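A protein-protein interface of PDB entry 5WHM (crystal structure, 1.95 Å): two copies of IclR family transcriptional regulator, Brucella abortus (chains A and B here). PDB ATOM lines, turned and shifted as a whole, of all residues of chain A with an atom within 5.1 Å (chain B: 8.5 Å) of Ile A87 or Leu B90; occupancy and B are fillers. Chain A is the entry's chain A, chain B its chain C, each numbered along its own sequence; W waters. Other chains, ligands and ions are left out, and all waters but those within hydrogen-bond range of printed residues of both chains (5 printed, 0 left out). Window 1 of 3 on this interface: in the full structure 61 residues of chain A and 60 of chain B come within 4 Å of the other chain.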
ATOM      1  N   LEU A  30      28.160  29.604 -24.442  1.00  0.00           N
ATOM      2  CA  LEU A  30      26.977  29.228 -23.651  1.00  0.00           C
ATOM      3  C   LEU A  30      26.457  27.835 -24.034  1.00  0.00           C
ATOM      4  O   LEU A  30      25.997  27.085 -23.160  1.00  0.00           O
ATOM      5  CB  LEU A  30      25.890  30.299 -23.793  1.00  0.00           C
ATOM      6  CG  LEU A  30      26.358  31.649 -23.210  1.00  0.00           C
ATOM      7  CD1 LEU A  30      25.389  32.808 -23.499  1.00  0.00           C
ATOM      8  CD2 LEU A  30      26.646  31.543 -21.701  1.00  0.00           C
ATOM      9  N   LEU A  33      28.172  25.137 -21.970  1.00  0.00           N
ATOM     10  CA  LEU A  33      27.602  24.924 -20.633  1.00  0.00           C
ATOM     11  C   LEU A  33      26.358  24.042 -20.693  1.00  0.00           C
ATOM     12  O   LEU A  33      26.119  23.227 -19.787  1.00  0.00           O
ATOM     13  CB  LEU A  33      27.259  26.264 -20.007  1.00  0.00           C
ATOM     14  CG  LEU A  33      28.455  27.213 -19.845  1.00  0.00           C
ATOM     15  CD1 LEU A  33      27.991  28.511 -19.218  1.00  0.00           C
ATOM     16  CD2 LEU A  33      29.475  26.556 -18.904  1.00  0.00           C
ATOM     17  N   ARG A  34      25.564  24.176 -21.758  1.00  0.00           N
ATOM     18  CA  ARG A  34      24.358  23.365 -21.938  1.00  0.00           C
ATOM     19  C   ARG A  34      24.630  21.898 -22.234  1.00  0.00           C
ATOM     20  O   ARG A  34      23.682  21.110 -22.157  1.00  0.00           O
ATOM     21  CB  ARG A  34      23.492  23.947 -23.062  1.00  0.00           C
ATOM     22  CG  ARG A  34      22.983  25.307 -22.684  1.00  0.00           C
ATOM     23  CD  ARG A  34      22.299  25.988 -23.842  1.00  0.00           C
ATOM     24  NE  ARG A  34      20.941  25.483 -23.969  1.00  0.00           N
ATOM     25  CZ  ARG A  34      19.859  26.240 -24.069  1.00  0.00           C
ATOM     26  NH1 ARG A  34      19.960  27.549 -24.101  1.00  0.00           N
ATOM     27  NH2 ARG A  34      18.679  25.671 -24.187  1.00  0.00           N
ATOM     28  N   TYR A  71      32.924  29.765 -14.729  1.00  0.00           N
ATOM     29  CA  TYR A  71      31.736  28.996 -15.080  1.00  0.00           C
ATOM     30  C   TYR A  71      32.009  27.500 -15.230  1.00  0.00           C
ATOM     31  O   TYR A  71      31.076  26.707 -15.097  1.00  0.00           O
ATOM     32  CB  TYR A  71      31.079  29.588 -16.349  1.00  0.00           C
ATOM     33  CG  TYR A  71      30.532  30.952 -16.011  1.00  0.00           C
ATOM     34  CD1 TYR A  71      29.363  31.071 -15.265  1.00  0.00           C
ATOM     35  CD2 TYR A  71      31.249  32.110 -16.301  1.00  0.00           C
ATOM     36  CE1 TYR A  71      28.876  32.317 -14.876  1.00  0.00           C
ATOM     37  CE2 TYR A  71      30.769  33.374 -15.920  1.00  0.00           C
ATOM     38  CZ  TYR A  71      29.580  33.463 -15.213  1.00  0.00           C
ATOM     39  OH  TYR A  71      29.101  34.687 -14.829  1.00  0.00           O
ATOM     40  N   LEU A  83      30.673  21.998 -14.248  1.00  0.00           N
ATOM     41  CA  LEU A  83      30.058  23.299 -14.034  1.00  0.00           C
ATOM     42  C   LEU A  83      30.537  23.876 -12.704  1.00  0.00           C
ATOM     43  O   LEU A  83      30.802  23.138 -11.762  1.00  0.00           O
ATOM     44  CB  LEU A  83      28.522  23.175 -14.037  1.00  0.00           C
ATOM     45  CG  LEU A  83      27.846  22.667 -15.324  1.00  0.00           C
ATOM     46  CD1 LEU A  83      26.311  22.556 -15.105  1.00  0.00           C
ATOM     47  CD2 LEU A  83      28.183  23.548 -16.536  1.00  0.00           C
ATOM     48  N   ASP A  84      30.672  25.200 -12.639  1.00  0.00           N
ATOM     49  CA  ASP A  84      31.054  25.855 -11.396  1.00  0.00           C
ATOM     50  C   ASP A  84      29.947  26.814 -10.956  1.00  0.00           C
ATOM     51  O   ASP A  84      28.983  27.064 -11.685  1.00  0.00           O
ATOM     52  CB  ASP A  84      32.392  26.579 -11.538  1.00  0.00           C
ATOM     53  CG  ASP A  84      33.136  26.707 -10.186  1.00  0.00           C
ATOM     54  OD1 ASP A  84      32.574  26.323  -9.123  1.00  0.00           O
ATOM     55  OD2 ASP A  84      34.288  27.180 -10.208  1.00  0.00           O
ATOM     56  N   ILE A  85      30.082  27.372  -9.750  1.00  0.00           N
ATOM     57  CA  ILE A  85      28.892  27.882  -9.074  1.00  0.00           C
ATOM     58  C   ILE A  85      28.460  29.272  -9.524  1.00  0.00           C
ATOM     59  O   ILE A  85      27.338  29.690  -9.193  1.00  0.00           O
ATOM     60  CB  ILE A  85      29.099  27.758  -7.554  1.00  0.00           C
ATOM     61  CG1 ILE A  85      30.463  28.286  -7.131  1.00  0.00           C
ATOM     62  CG2 ILE A  85      28.989  26.292  -7.155  1.00  0.00           C
ATOM     63  CD1 ILE A  85      30.545  29.748  -7.130  1.00  0.00           C
ATOM     64  N   GLY A  86      29.282  29.977 -10.288  1.00  0.00           N
ATOM     65  CA  GLY A  86      28.823  31.129 -11.054  1.00  0.00           C
ATOM     66  C   GLY A  86      27.511  30.902 -11.810  1.00  0.00           C
ATOM     67  O   GLY A  86      26.704  31.830 -11.979  1.00  0.00           O
ATOM     68  N   ILE A  87      27.298  29.676 -12.291  1.00  0.00           N
ATOM     69  CA  ILE A  87      26.062  29.364 -13.013  1.00  0.00           C
ATOM     70  C   ILE A  87      24.866  29.401 -12.068  1.00  0.00           C
ATOM     71  O   ILE A  87      23.758  29.820 -12.449  1.00  0.00           O
ATOM     72  CB  ILE A  87      26.215  27.996 -13.697  1.00  0.00           C
ATOM     73  CG1 ILE A  87      27.170  28.143 -14.900  1.00  0.00           C
ATOM     74  CG2 ILE A  87      24.857  27.452 -14.143  1.00  0.00           C
ATOM     75  CD1 ILE A  87      27.656  26.857 -15.438  1.00  0.00           C
ATOM     76  N   LEU A  88      25.067  28.968 -10.811  1.00  0.00           N
ATOM     77  CA  LEU A  88      23.971  29.009  -9.853  1.00  0.00           C
ATOM     78  C   LEU A  88      23.611  30.450  -9.533  1.00  0.00           C
ATOM     79  O   LEU A  88      22.435  30.800  -9.360  1.00  0.00           O
ATOM     80  CB  LEU A  88      24.356  28.215  -8.591  1.00  0.00           C
ATOM     81  CG  LEU A  88      23.262  27.942  -7.566  1.00  0.00           C
ATOM     82  CD1 LEU A  88      22.328  26.871  -8.118  1.00  0.00           C
ATOM     83  CD2 LEU A  88      23.903  27.428  -6.233  1.00  0.00           C
ATOM     84  N   ARG A  89      24.607  31.313  -9.491  1.00  0.00           N
ATOM     85  CA  ARG A  89      24.360  32.717  -9.185  1.00  0.00           C
ATOM     86  C   ARG A  89      23.562  33.377 -10.305  1.00  0.00           C
ATOM     87  O   ARG A  89      22.650  34.178 -10.050  1.00  0.00           O
ATOM     88  CB  ARG A  89      25.708  33.415  -8.996  1.00  0.00           C
ATOM     89  CG  ARG A  89      25.633  34.854  -8.595  1.00  0.00           C
ATOM     90  CD  ARG A  89      27.053  35.423  -8.481  1.00  0.00           C
ATOM     91  NE  ARG A  89      26.979  36.798  -8.007  1.00  0.00           N
ATOM     92  CZ  ARG A  89      28.015  37.561  -7.658  1.00  0.00           C
ATOM     93  NH1 ARG A  89      27.769  38.782  -7.220  1.00  0.00           N
ATOM     94  NH2 ARG A  89      29.266  37.110  -7.687  1.00  0.00           N
ATOM     95  N   LEU A  90      23.940  33.092 -11.550  1.00  0.00           N
ATOM     96  CA  LEU A  90      23.187  33.571 -12.699  1.00  0.00           C
ATOM     97  C   LEU A  90      21.723  33.090 -12.654  1.00  0.00           C
ATOM     98  O   LEU A  90      20.799  33.870 -12.886  1.00  0.00           O
ATOM     99  CB  LEU A  90      23.880  33.044 -13.957  1.00  0.00           C
ATOM    100  CG  LEU A  90      24.051  33.861 -15.224  1.00  0.00           C
ATOM    101  CD1 LEU A  90      24.601  35.203 -14.881  1.00  0.00           C
ATOM    102  CD2 LEU A  90      25.000  33.099 -16.183  1.00  0.00           C
ATOM    103  N   GLY A  91      21.497  31.814 -12.335  1.00  0.00           N
ATOM    104  CA  GLY A  91      20.130  31.285 -12.320  1.00  0.00           C
ATOM    105  C   GLY A  91      19.249  31.948 -11.288  1.00  0.00           C
ATOM    106  O   GLY A  91      18.079  32.259 -11.554  1.00  0.00           O
ATOM    107  N   LEU B  30      29.424  37.259 -21.013  1.00  0.00           N
ATOM    108  CA  LEU B  30      29.135  36.816 -19.644  1.00  0.00           C
ATOM    109  C   LEU B  30      29.201  37.984 -18.667  1.00  0.00           C
ATOM    110  O   LEU B  30      28.426  38.028 -17.699  1.00  0.00           O
ATOM    111  CB  LEU B  30      30.106  35.721 -19.219  1.00  0.00           C
ATOM    112  CG  LEU B  30      29.821  34.403 -19.954  1.00  0.00           C
ATOM    113  CD1 LEU B  30      31.017  33.493 -19.848  1.00  0.00           C
ATOM    114  CD2 LEU B  30      28.631  33.721 -19.335  1.00  0.00           C
ATOM    115  N   LEU B  33      25.855  39.503 -18.842  1.00  0.00           N
ATOM    116  CA  LEU B  33      24.876  38.757 -18.046  1.00  0.00           C
ATOM    117  C   LEU B  33      25.091  38.969 -16.551  1.00  0.00           C
ATOM    118  O   LEU B  33      24.121  38.983 -15.785  1.00  0.00           O
ATOM    119  CB  LEU B  33      24.942  37.264 -18.363  1.00  0.00           C
ATOM    120  CG  LEU B  33      24.431  36.868 -19.748  1.00  0.00           C
ATOM    121  CD1 LEU B  33      24.772  35.391 -20.009  1.00  0.00           C
ATOM    122  CD2 LEU B  33      22.907  37.141 -19.828  1.00  0.00           C
ATOM    123  N   ARG B  34      26.341  39.178 -16.120  1.00  0.00           N
ATOM    124  CA  ARG B  34      26.588  39.424 -14.690  1.00  0.00           C
ATOM    125  C   ARG B  34      26.084  40.784 -14.216  1.00  0.00           C
ATOM    126  O   ARG B  34      26.075  41.026 -12.999  1.00  0.00           O
ATOM    127  CB  ARG B  34      28.079  39.328 -14.373  1.00  0.00           C
ATOM    128  CG  ARG B  34      28.668  37.930 -14.399  1.00  0.00           C
ATOM    129  CD  ARG B  34      30.091  37.978 -13.802  1.00  0.00           C
ATOM    130  NE  ARG B  34      30.705  36.657 -13.672  1.00  0.00           N
ATOM    131  CZ  ARG B  34      30.804  35.977 -12.527  1.00  0.00           C
ATOM    132  NH1 ARG B  34      31.388  34.772 -12.509  1.00  0.00           N
ATOM    133  NH2 ARG B  34      30.332  36.503 -11.400  1.00  0.00           N
ATOM    134  N   LEU B  66      22.180  37.705 -27.106  1.00  0.00           N
ATOM    135  CA  LEU B  66      21.606  37.015 -25.953  1.00  0.00           C
ATOM    136  C   LEU B  66      20.086  36.912 -26.081  1.00  0.00           C
ATOM    137  O   LEU B  66      19.493  35.899 -25.693  1.00  0.00           O
ATOM    138  CB  LEU B  66      22.026  37.740 -24.650  1.00  0.00           C
ATOM    139  CG  LEU B  66      23.524  37.611 -24.356  1.00  0.00           C
ATOM    140  CD1 LEU B  66      23.990  38.632 -23.250  1.00  0.00           C
ATOM    141  CD2 LEU B  66      23.856  36.176 -23.931  1.00  0.00           C
ATOM    142  N   GLY B  70      17.744  33.406 -26.307  1.00  0.00           N
ATOM    143  CA  GLY B  70      16.839  33.103 -25.209  1.00  0.00           C
ATOM    144  C   GLY B  70      17.414  33.310 -23.820  1.00  0.00           C
ATOM    145  O   GLY B  70      16.779  32.883 -22.853  1.00  0.00           O
ATOM    146  N   TYR B  71      18.604  33.923 -23.688  1.00  0.00           N
ATOM    147  CA  TYR B  71      19.164  34.241 -22.358  1.00  0.00           C
ATOM    148  C   TYR B  71      18.727  35.597 -21.837  1.00  0.00           C
ATOM    149  O   TYR B  71      18.775  35.832 -20.619  1.00  0.00           O
ATOM    150  CB  TYR B  71      20.699  34.225 -22.383  1.00  0.00           C
ATOM    151  CG  TYR B  71      21.220  32.893 -22.843  1.00  0.00           C
ATOM    152  CD1 TYR B  71      21.024  31.742 -22.064  1.00  0.00           C
ATOM    153  CD2 TYR B  71      21.915  32.776 -24.057  1.00  0.00           C
ATOM    154  CE1 TYR B  71      21.473  30.503 -22.495  1.00  0.00           C
ATOM    155  CE2 TYR B  71      22.374  31.535 -24.493  1.00  0.00           C
ATOM    156  CZ  TYR B  71      22.145  30.410 -23.697  1.00  0.00           C
ATOM    157  OH  TYR B  71      22.605  29.173 -24.099  1.00  0.00           O
ATOM    158  N   LEU B  83      16.928  39.023 -17.669  1.00  0.00           N
ATOM    159  CA  LEU B  83      17.350  37.630 -17.838  1.00  0.00           C
ATOM    160  C   LEU B  83      16.135  36.782 -18.225  1.00  0.00           C
ATOM    161  O   LEU B  83      15.028  36.996 -17.724  1.00  0.00           O
ATOM    162  CB  LEU B  83      17.955  37.065 -16.535  1.00  0.00           C
ATOM    163  CG  LEU B  83      19.282  37.740 -16.107  1.00  0.00           C
ATOM    164  CD1 LEU B  83      19.690  37.207 -14.718  1.00  0.00           C
ATOM    165  CD2 LEU B  83      20.376  37.474 -17.143  1.00  0.00           C
ATOM    166  N   ASP B  84      16.362  35.762 -19.054  1.00  0.00           N
ATOM    167  CA  ASP B  84      15.258  34.908 -19.469  1.00  0.00           C
ATOM    168  C   ASP B  84      15.570  33.434 -19.176  1.00  0.00           C
ATOM    169  O   ASP B  84      16.662  33.072 -18.708  1.00  0.00           O
ATOM    170  CB  ASP B  84      14.930  35.140 -20.960  1.00  0.00           C
ATOM    171  CG  ASP B  84      13.480  34.751 -21.335  1.00  0.00           C
ATOM    172  OD1 ASP B  84      12.687  34.263 -20.491  1.00  0.00           O
ATOM    173  OD2 ASP B  84      13.144  34.965 -22.519  1.00  0.00           O
ATOM    174  N   ILE B  85      14.569  32.595 -19.483  1.00  0.00           N
ATOM    175  CA  ILE B  85      14.509  31.192 -19.065  1.00  0.00           C
ATOM    176  C   ILE B  85      15.741  30.424 -19.495  1.00  0.00           C
ATOM    177  O   ILE B  85      16.156  29.470 -18.821  1.00  0.00           O
ATOM    178  CB  ILE B  85      13.256  30.498 -19.661  1.00  0.00           C
ATOM    179  CG1 ILE B  85      11.982  31.305 -19.377  1.00  0.00           C
ATOM    180  CG2 ILE B  85      13.160  29.041 -19.137  1.00  0.00           C
ATOM    181  CD1 ILE B  85      11.815  31.688 -17.885  1.00  0.00           C
ATOM    182  N   GLY B  86      16.313  30.767 -20.651  1.00  0.00           N
ATOM    183  CA  GLY B  86      17.456  30.002 -21.097  1.00  0.00           C
ATOM    184  C   GLY B  86      18.624  30.054 -20.136  1.00  0.00           C
ATOM    185  O   GLY B  86      19.465  29.154 -20.157  1.00  0.00           O
ATOM    186  N   ILE B  87      18.662  31.047 -19.246  1.00  0.00           N
ATOM    187  CA  ILE B  87      19.738  31.078 -18.235  1.00  0.00           C
ATOM    188  C   ILE B  87      19.734  29.790 -17.406  1.00  0.00           C
ATOM    189  O   ILE B  87      20.796  29.255 -17.051  1.00  0.00           O
ATOM    190  CB  ILE B  87      19.593  32.331 -17.340  1.00  0.00           C
ATOM    191  CG1 ILE B  87      19.831  33.627 -18.139  1.00  0.00           C
ATOM    192  CG2 ILE B  87      20.538  32.295 -16.112  1.00  0.00           C
ATOM    193  CD1 ILE B  87      21.316  33.846 -18.539  1.00  0.00           C
ATOM    194  N   LEU B  88      18.544  29.250 -17.104  1.00  0.00           N
ATOM    195  CA  LEU B  88      18.492  28.058 -16.239  1.00  0.00           C
ATOM    196  C   LEU B  88      19.040  26.808 -16.911  1.00  0.00           C
ATOM    197  O   LEU B  88      19.472  25.884 -16.215  1.00  0.00           O
ATOM    198  CB  LEU B  88      17.053  27.790 -15.742  1.00  0.00           C
ATOM    199  CG  LEU B  88      16.427  28.949 -14.970  1.00  0.00           C
ATOM    200  CD1 LEU B  88      14.940  28.685 -14.686  1.00  0.00           C
ATOM    201  CD2 LEU B  88      17.178  29.187 -13.643  1.00  0.00           C
ATOM    202  N   ARG B  89      19.064  26.764 -18.232  1.00  0.00           N
ATOM    203  CA  ARG B  89      19.587  25.619 -18.970  1.00  0.00           C
ATOM    204  C   ARG B  89      21.113  25.559 -18.936  1.00  0.00           C
ATOM    205  O   ARG B  89      21.699  24.596 -19.446  1.00  0.00           O
ATOM    206  CB  ARG B  89      19.156  25.690 -20.448  1.00  0.00           C
ATOM    207  CG  ARG B  89      17.661  25.882 -20.758  1.00  0.00           C
ATOM    208  CD  ARG B  89      16.856  24.637 -20.398  1.00  0.00           C
ATOM    209  NE  ARG B  89      17.229  23.378 -21.079  1.00  0.00           N
ATOM    210  CZ  ARG B  89      16.769  22.946 -22.261  1.00  0.00           C
ATOM    211  NH1 ARG B  89      17.141  21.751 -22.710  1.00  0.00           N
ATOM    212  NH2 ARG B  89      15.975  23.692 -23.028  1.00  0.00           N
ATOM    213  N   LEU B  90      21.768  26.610 -18.467  1.00  0.00           N
ATOM    214  CA  LEU B  90      23.216  26.567 -18.291  1.00  0.00           C
ATOM    215  C   LEU B  90      23.644  25.700 -17.108  1.00  0.00           C
ATOM    216  O   LEU B  90      24.850  25.456 -16.935  1.00  0.00           O
ATOM    217  CB  LEU B  90      23.749  27.988 -18.101  1.00  0.00           C
ATOM    218  CG  LEU B  90      23.403  28.973 -19.243  1.00  0.00           C
ATOM    219  CD1 LEU B  90      23.832  30.407 -18.861  1.00  0.00           C
ATOM    220  CD2 LEU B  90      24.044  28.539 -20.536  1.00  0.00           C
ATOM    221  N   GLY B  91      22.707  25.253 -16.279  1.00  0.00           N
ATOM    222  CA  GLY B  91      23.032  24.268 -15.254  1.00  0.00           C
ATOM    223  C   GLY B  91      22.514  24.541 -13.850  1.00  0.00           C
ATOM    224  O   GLY B  91      22.988  23.891 -12.909  1.00  0.00           O
ATOM    225  N   TYR B  92      21.541  25.450 -13.679  1.00  0.00           N
ATOM    226  CA  TYR B  92      21.083  25.793 -12.324  1.00  0.00           C
ATOM    227  C   TYR B  92      20.650  24.556 -11.514  1.00  0.00           C
ATOM    228  O   TYR B  92      21.072  24.385 -10.357  1.00  0.00           O
ATOM    229  CB  TYR B  92      19.934  26.812 -12.401  1.00  0.00           C
ATOM    230  CG  TYR B  92      19.364  27.180 -11.047  1.00  0.00           C
ATOM    231  CD1 TYR B  92      19.924  28.211 -10.293  1.00  0.00           C
ATOM    232  CD2 TYR B  92      18.273  26.491 -10.519  1.00  0.00           C
ATOM    233  CE1 TYR B  92      19.412  28.567  -9.038  1.00  0.00           C
ATOM    234  CE2 TYR B  92      17.765  26.824  -9.262  1.00  0.00           C
ATOM    235  CZ  TYR B  92      18.362  27.848  -8.525  1.00  0.00           C
ATOM    236  OH  TYR B  92      17.826  28.175  -7.327  1.00  0.00           O
ATOM    237  N   ALA B  93      19.784  23.695 -12.089  1.00  0.00           N
ATOM    238  CA  ALA B  93      19.260  22.553 -11.320  1.00  0.00           C
ATOM    239  C   ALA B  93      20.360  21.567 -10.896  1.00  0.00           C
ATOM    240  O   ALA B  93      20.350  21.040  -9.779  1.00  0.00           O
ATOM    241  CB  ALA B  93      18.181  21.836 -12.127  1.00  0.00           C
ATOM    242  N   MET B  94      21.291  21.269 -11.781  1.00  0.00           N
ATOM    243  CA  MET B  94      22.388  20.390 -11.406  1.00  0.00           C
ATOM    244  C   MET B  94      23.218  20.967 -10.250  1.00  0.00           C
ATOM    245  O   MET B  94      23.595  20.248  -9.343  1.00  0.00           O
ATOM    246  CB  MET B  94      23.306  20.152 -12.606  1.00  0.00           C
ATOM    247  CG  MET B  94      22.650  19.361 -13.702  1.00  0.00           C
ATOM    248  SD  MET B  94      23.795  19.482 -15.297  1.00  0.00           S
ATOM    249  CE  MET B  94      25.459  18.985 -14.537  1.00  0.00           C
ATOM    250  N   LEU B  95      23.483  22.274 -10.278  1.00  0.00           N
ATOM    251  CA  LEU B  95      24.289  22.862  -9.205  1.00  0.00           C
ATOM    252  C   LEU B  95      23.505  22.985  -7.901  1.00  0.00           C
ATOM    253  O   LEU B  95      24.109  23.085  -6.830  1.00  0.00           O
ATOM    254  CB  LEU B  95      24.810  24.235  -9.634  1.00  0.00           C
ATOM    255  CG  LEU B  95      25.938  24.034 -10.677  1.00  0.00           C
ATOM    256  CD1 LEU B  95      26.128  25.271 -11.462  1.00  0.00           C
ATOM    257  CD2 LEU B  95      27.249  23.673  -9.976  1.00  0.00           C
ATOM    258  N   SER B  96      22.178  23.004  -7.968  1.00  0.00           N
ATOM    259  CA  SER B  96      21.378  22.954  -6.749  1.00  0.00           C
ATOM    260  C   SER B  96      21.338  21.552  -6.161  1.00  0.00           C
ATOM    261  O   SER B  96      20.776  21.361  -5.082  1.00  0.00           O
ATOM    262  CB  SER B  96      19.955  23.438  -7.077  1.00  0.00           C
ATOM    263  OG  SER B  96      19.215  22.396  -7.726  1.00  0.00           O
ATOM    264  N   ASP B 125      32.240  32.992  -5.422  1.00  0.00           N
ATOM    265  CA  ASP B 125      32.273  33.421  -6.830  1.00  0.00           C
ATOM    266  C   ASP B 125      32.675  34.894  -6.840  1.00  0.00           C
ATOM    267  O   ASP B 125      31.918  35.748  -6.359  1.00  0.00           O
ATOM    268  CB  ASP B 125      30.922  33.197  -7.555  1.00  0.00           C
ATOM    269  CG  ASP B 125      30.919  33.782  -9.012  1.00  0.00           C
ATOM    270  OD1 ASP B 125      30.295  34.836  -9.272  1.00  0.00           O
ATOM    271  OD2 ASP B 125      31.574  33.188  -9.904  1.00  0.00           O
ATOM    272  N   VAL B 130      28.297  32.307  -2.506  1.00  0.00           N
ATOM    273  CA  VAL B 130      27.051  31.854  -3.111  1.00  0.00           C
ATOM    274  C   VAL B 130      26.526  30.683  -2.285  1.00  0.00           C
ATOM    275  O   VAL B 130      27.223  29.681  -2.119  1.00  0.00           O
ATOM    276  CB  VAL B 130      27.280  31.412  -4.573  1.00  0.00           C
ATOM    277  CG1 VAL B 130      25.959  31.024  -5.227  1.00  0.00           C
ATOM    278  CG2 VAL B 130      27.998  32.531  -5.362  1.00  0.00           C
ATOM    279  N   ILE B 147      18.762  29.515  -2.699  1.00  0.00           N
ATOM    280  CA  ILE B 147      19.827  28.806  -3.398  1.00  0.00           C
ATOM    281  C   ILE B 147      20.366  29.721  -4.493  1.00  0.00           C
ATOM    282  O   ILE B 147      19.624  30.120  -5.395  1.00  0.00           O
ATOM    283  CB  ILE B 147      19.282  27.494  -3.998  1.00  0.00           C
ATOM    284  CG1 ILE B 147      18.586  26.666  -2.917  1.00  0.00           C
ATOM    285  CG2 ILE B 147      20.383  26.688  -4.687  1.00  0.00           C
ATOM    286  CD1 ILE B 147      19.502  26.262  -1.814  1.00  0.00           C
ATOM    287  N   GLY B 148      21.661  30.025  -4.449  1.00  0.00           N
ATOM    288  CA  GLY B 148      22.239  30.946  -5.407  1.00  0.00           C
ATOM    289  C   GLY B 148      22.234  32.406  -4.989  1.00  0.00           C
ATOM    290  O   GLY B 148      22.801  33.226  -5.708  1.00  0.00           O
HETATM  291  O   HOH W   1      21.592  28.807 -14.411  1.00  0.00           O
HETATM  292  O   HOH W   2      23.753  22.406 -18.372  1.00  0.00           O
HETATM  293  O   HOH W   3      32.158  30.562 -10.034  1.00  0.00           O
HETATM  294  O   HOH W   4      20.037  22.754 -23.192  1.00  0.00           O
HETATM  295  O   HOH W   5      21.005  22.333 -20.833  1.00  0.00           O
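O of Ala B93 is in hydrogen-bond range of OG of Ser B96, 2.7 Å away.
The backbone carbonyl oxygen (O) of Tyr B71 lies within hydrogen-bond range of the backbone NH (N) of Asp B84 (2.9 Å).
The backbone carbonyl oxygen of Ile B147 is in hydrogen-bond range of the side-chain hydroxyl of Tyr B92 (3.3 Å).
NH2 of Arg B34 lies within salt-bridge range of OD1 of Asp B125 (2.7 Å).
The backbone carbonyl oxygen (O) of Tyr A71 is in hydrogen-bond range of the backbone NH (N) of Asp A84.
O of Leu B66 sits at hydrogen-bond distance from N of Tyr B71 (3.0 Å).
Leu A30 touches its own counterpart, Leu B30.
Leu A30 touches Leu B90, but with the chains exchanged Leu A90 does not touch Leu B30 (4.8 Å).
Ile A87 touches Leu B90, and with the chains exchanged Leu A90 touches Ile B87.
Ile A87 touches Gly B91, and with the chains exchanged Gly A91 touches Ile B87.
13 positions are printed for both chains.
Of the 34 pairs that touch across the chains among the printed residues, 16 have their exchanged pair printed and touching as well.
Leu B30 touches Leu A30 (CD2 to CD2, 3.8 Å).
Leu A30 touches Tyr B71.
CD1 of Leu A83 touches CE of Met B94 (3.7 Å).
Arg A89 touches Arg B34.
Arg A89 touches Gly B148.
Leu B33 touches Leu A90 (O to CD1, 3.9 Å).
Leu A90 touches Leu B83 (O to CD1, 3.97 Å).
CD2 of Leu A90 touches CD1 of Leu B90 (3.97 Å).
Leu B88 touches Gly A91.
Gly A91 touches Tyr B92.
Of the 13 printed residues of chain A, 13 touch a printed residue of chain B.
Printed residues of chain A that touch a printed residue of chain B: Leu A30, Leu A33, Arg A34, Tyr A71, Leu A83, Asp A84, Ile A85, Gly A86, Ile A87, Leu A88, Arg A89, Leu A90 and Gly A91.
Hydrophobic or aromatic side chains of chain A within 4 Å of the printed part of chain B: Leu A30, Leu A33, Tyr A71, Leu A83, Ile A85, Ile A87, Leu A88 and Leu A90.
Of the 24 printed residues of chain B, 18 touch a printed residue of chain A.
Printed residues of chain B that touch a printed residue of chain A: Leu B30, Leu B33, Arg B34, Leu B66, Tyr B71, Leu B83, Ile B87, Leu B88, Arg B89, Leu B90, Gly B91, Tyr B92, Met B94, Leu B95, Ser B96, Asp B125, Ile B147 and Gly B148.
Among the printed residues, Asp or Glu carboxylates within 4 Å of a Lys or Arg side-chain nitrogen of the other chain: Arg A89 with Asp B125 (3.0 Å).
Gly A86 touches just one residue of chain B: Asp B125 (3.6 Å).
Ile A87 touches just these residues of chain B: Leu B90 (3.4 Å), Gly B91 (3.7 Å), Tyr B92 (3.9 Å) and Leu B95 (3.5 Å).
Printed residues of chain B within 4 Å of Leu A88: Tyr B92, Leu B95, Ser B96, Ile B147 and Gly B148.
Gly B70 touches none of the printed residues of chain A.
Gly B86 touches none of the printed residues of chain A.
Printed residues of chain A within 4 Å of Ile B87: Leu A90 (3.6 Å) and Gly A91 (3.9 Å).
Printed residues of chain A within 4 Å of Arg B89: Arg A34 (3.5 Å).
Leu B90 touches just these residues of chain A: Leu A30, Leu A33, Leu A83, Ile A87 and Leu A90.
Of the printed residues of chain A, Ile B147 touches Leu A88.
The nearest residue of chain B that does not touch Ile A87 is Ile B87 (5.3 Å).
Water W3 bridges the side-chain carboxylate (OD2) of Asp B125 (2.7 Å) and the backbone NH (N) of Gly A86 (2.9 Å).
Water W5 lies within hydrogen-bond range of the backbone carbonyl oxygen of Arg B89 (2.7 Å) and the backbone carbonyl oxygen of Arg A34 (3.2 Å).
Water W1 lies within hydrogen-bond range of the backbone carbonyl oxygen (O) of Ile B87 (2.8 Å), the backbone carbonyl oxygen (O) of Ile A87 (3.1 Å) and the backbone NH (N) of Tyr B92 (3.4 Å).
Water W2 bridges O of Leu A33 and O of Arg B89.
Water W4 bridges NE of Arg A34 (3.0 Å) and NH1 of Arg B89 (3.1 Å).
NH2 of Arg A89 is in salt-bridge range of OD1 of Asp B125 (3.0 Å).
The guanidinium group (NH1) of Arg A34 sits at hydrogen-bond distance from the side-chain hydroxyl (OH) of Tyr B71.
OH of Tyr A71 sits at hydrogen-bond distance from NE of Arg B34 (2.8 Å).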
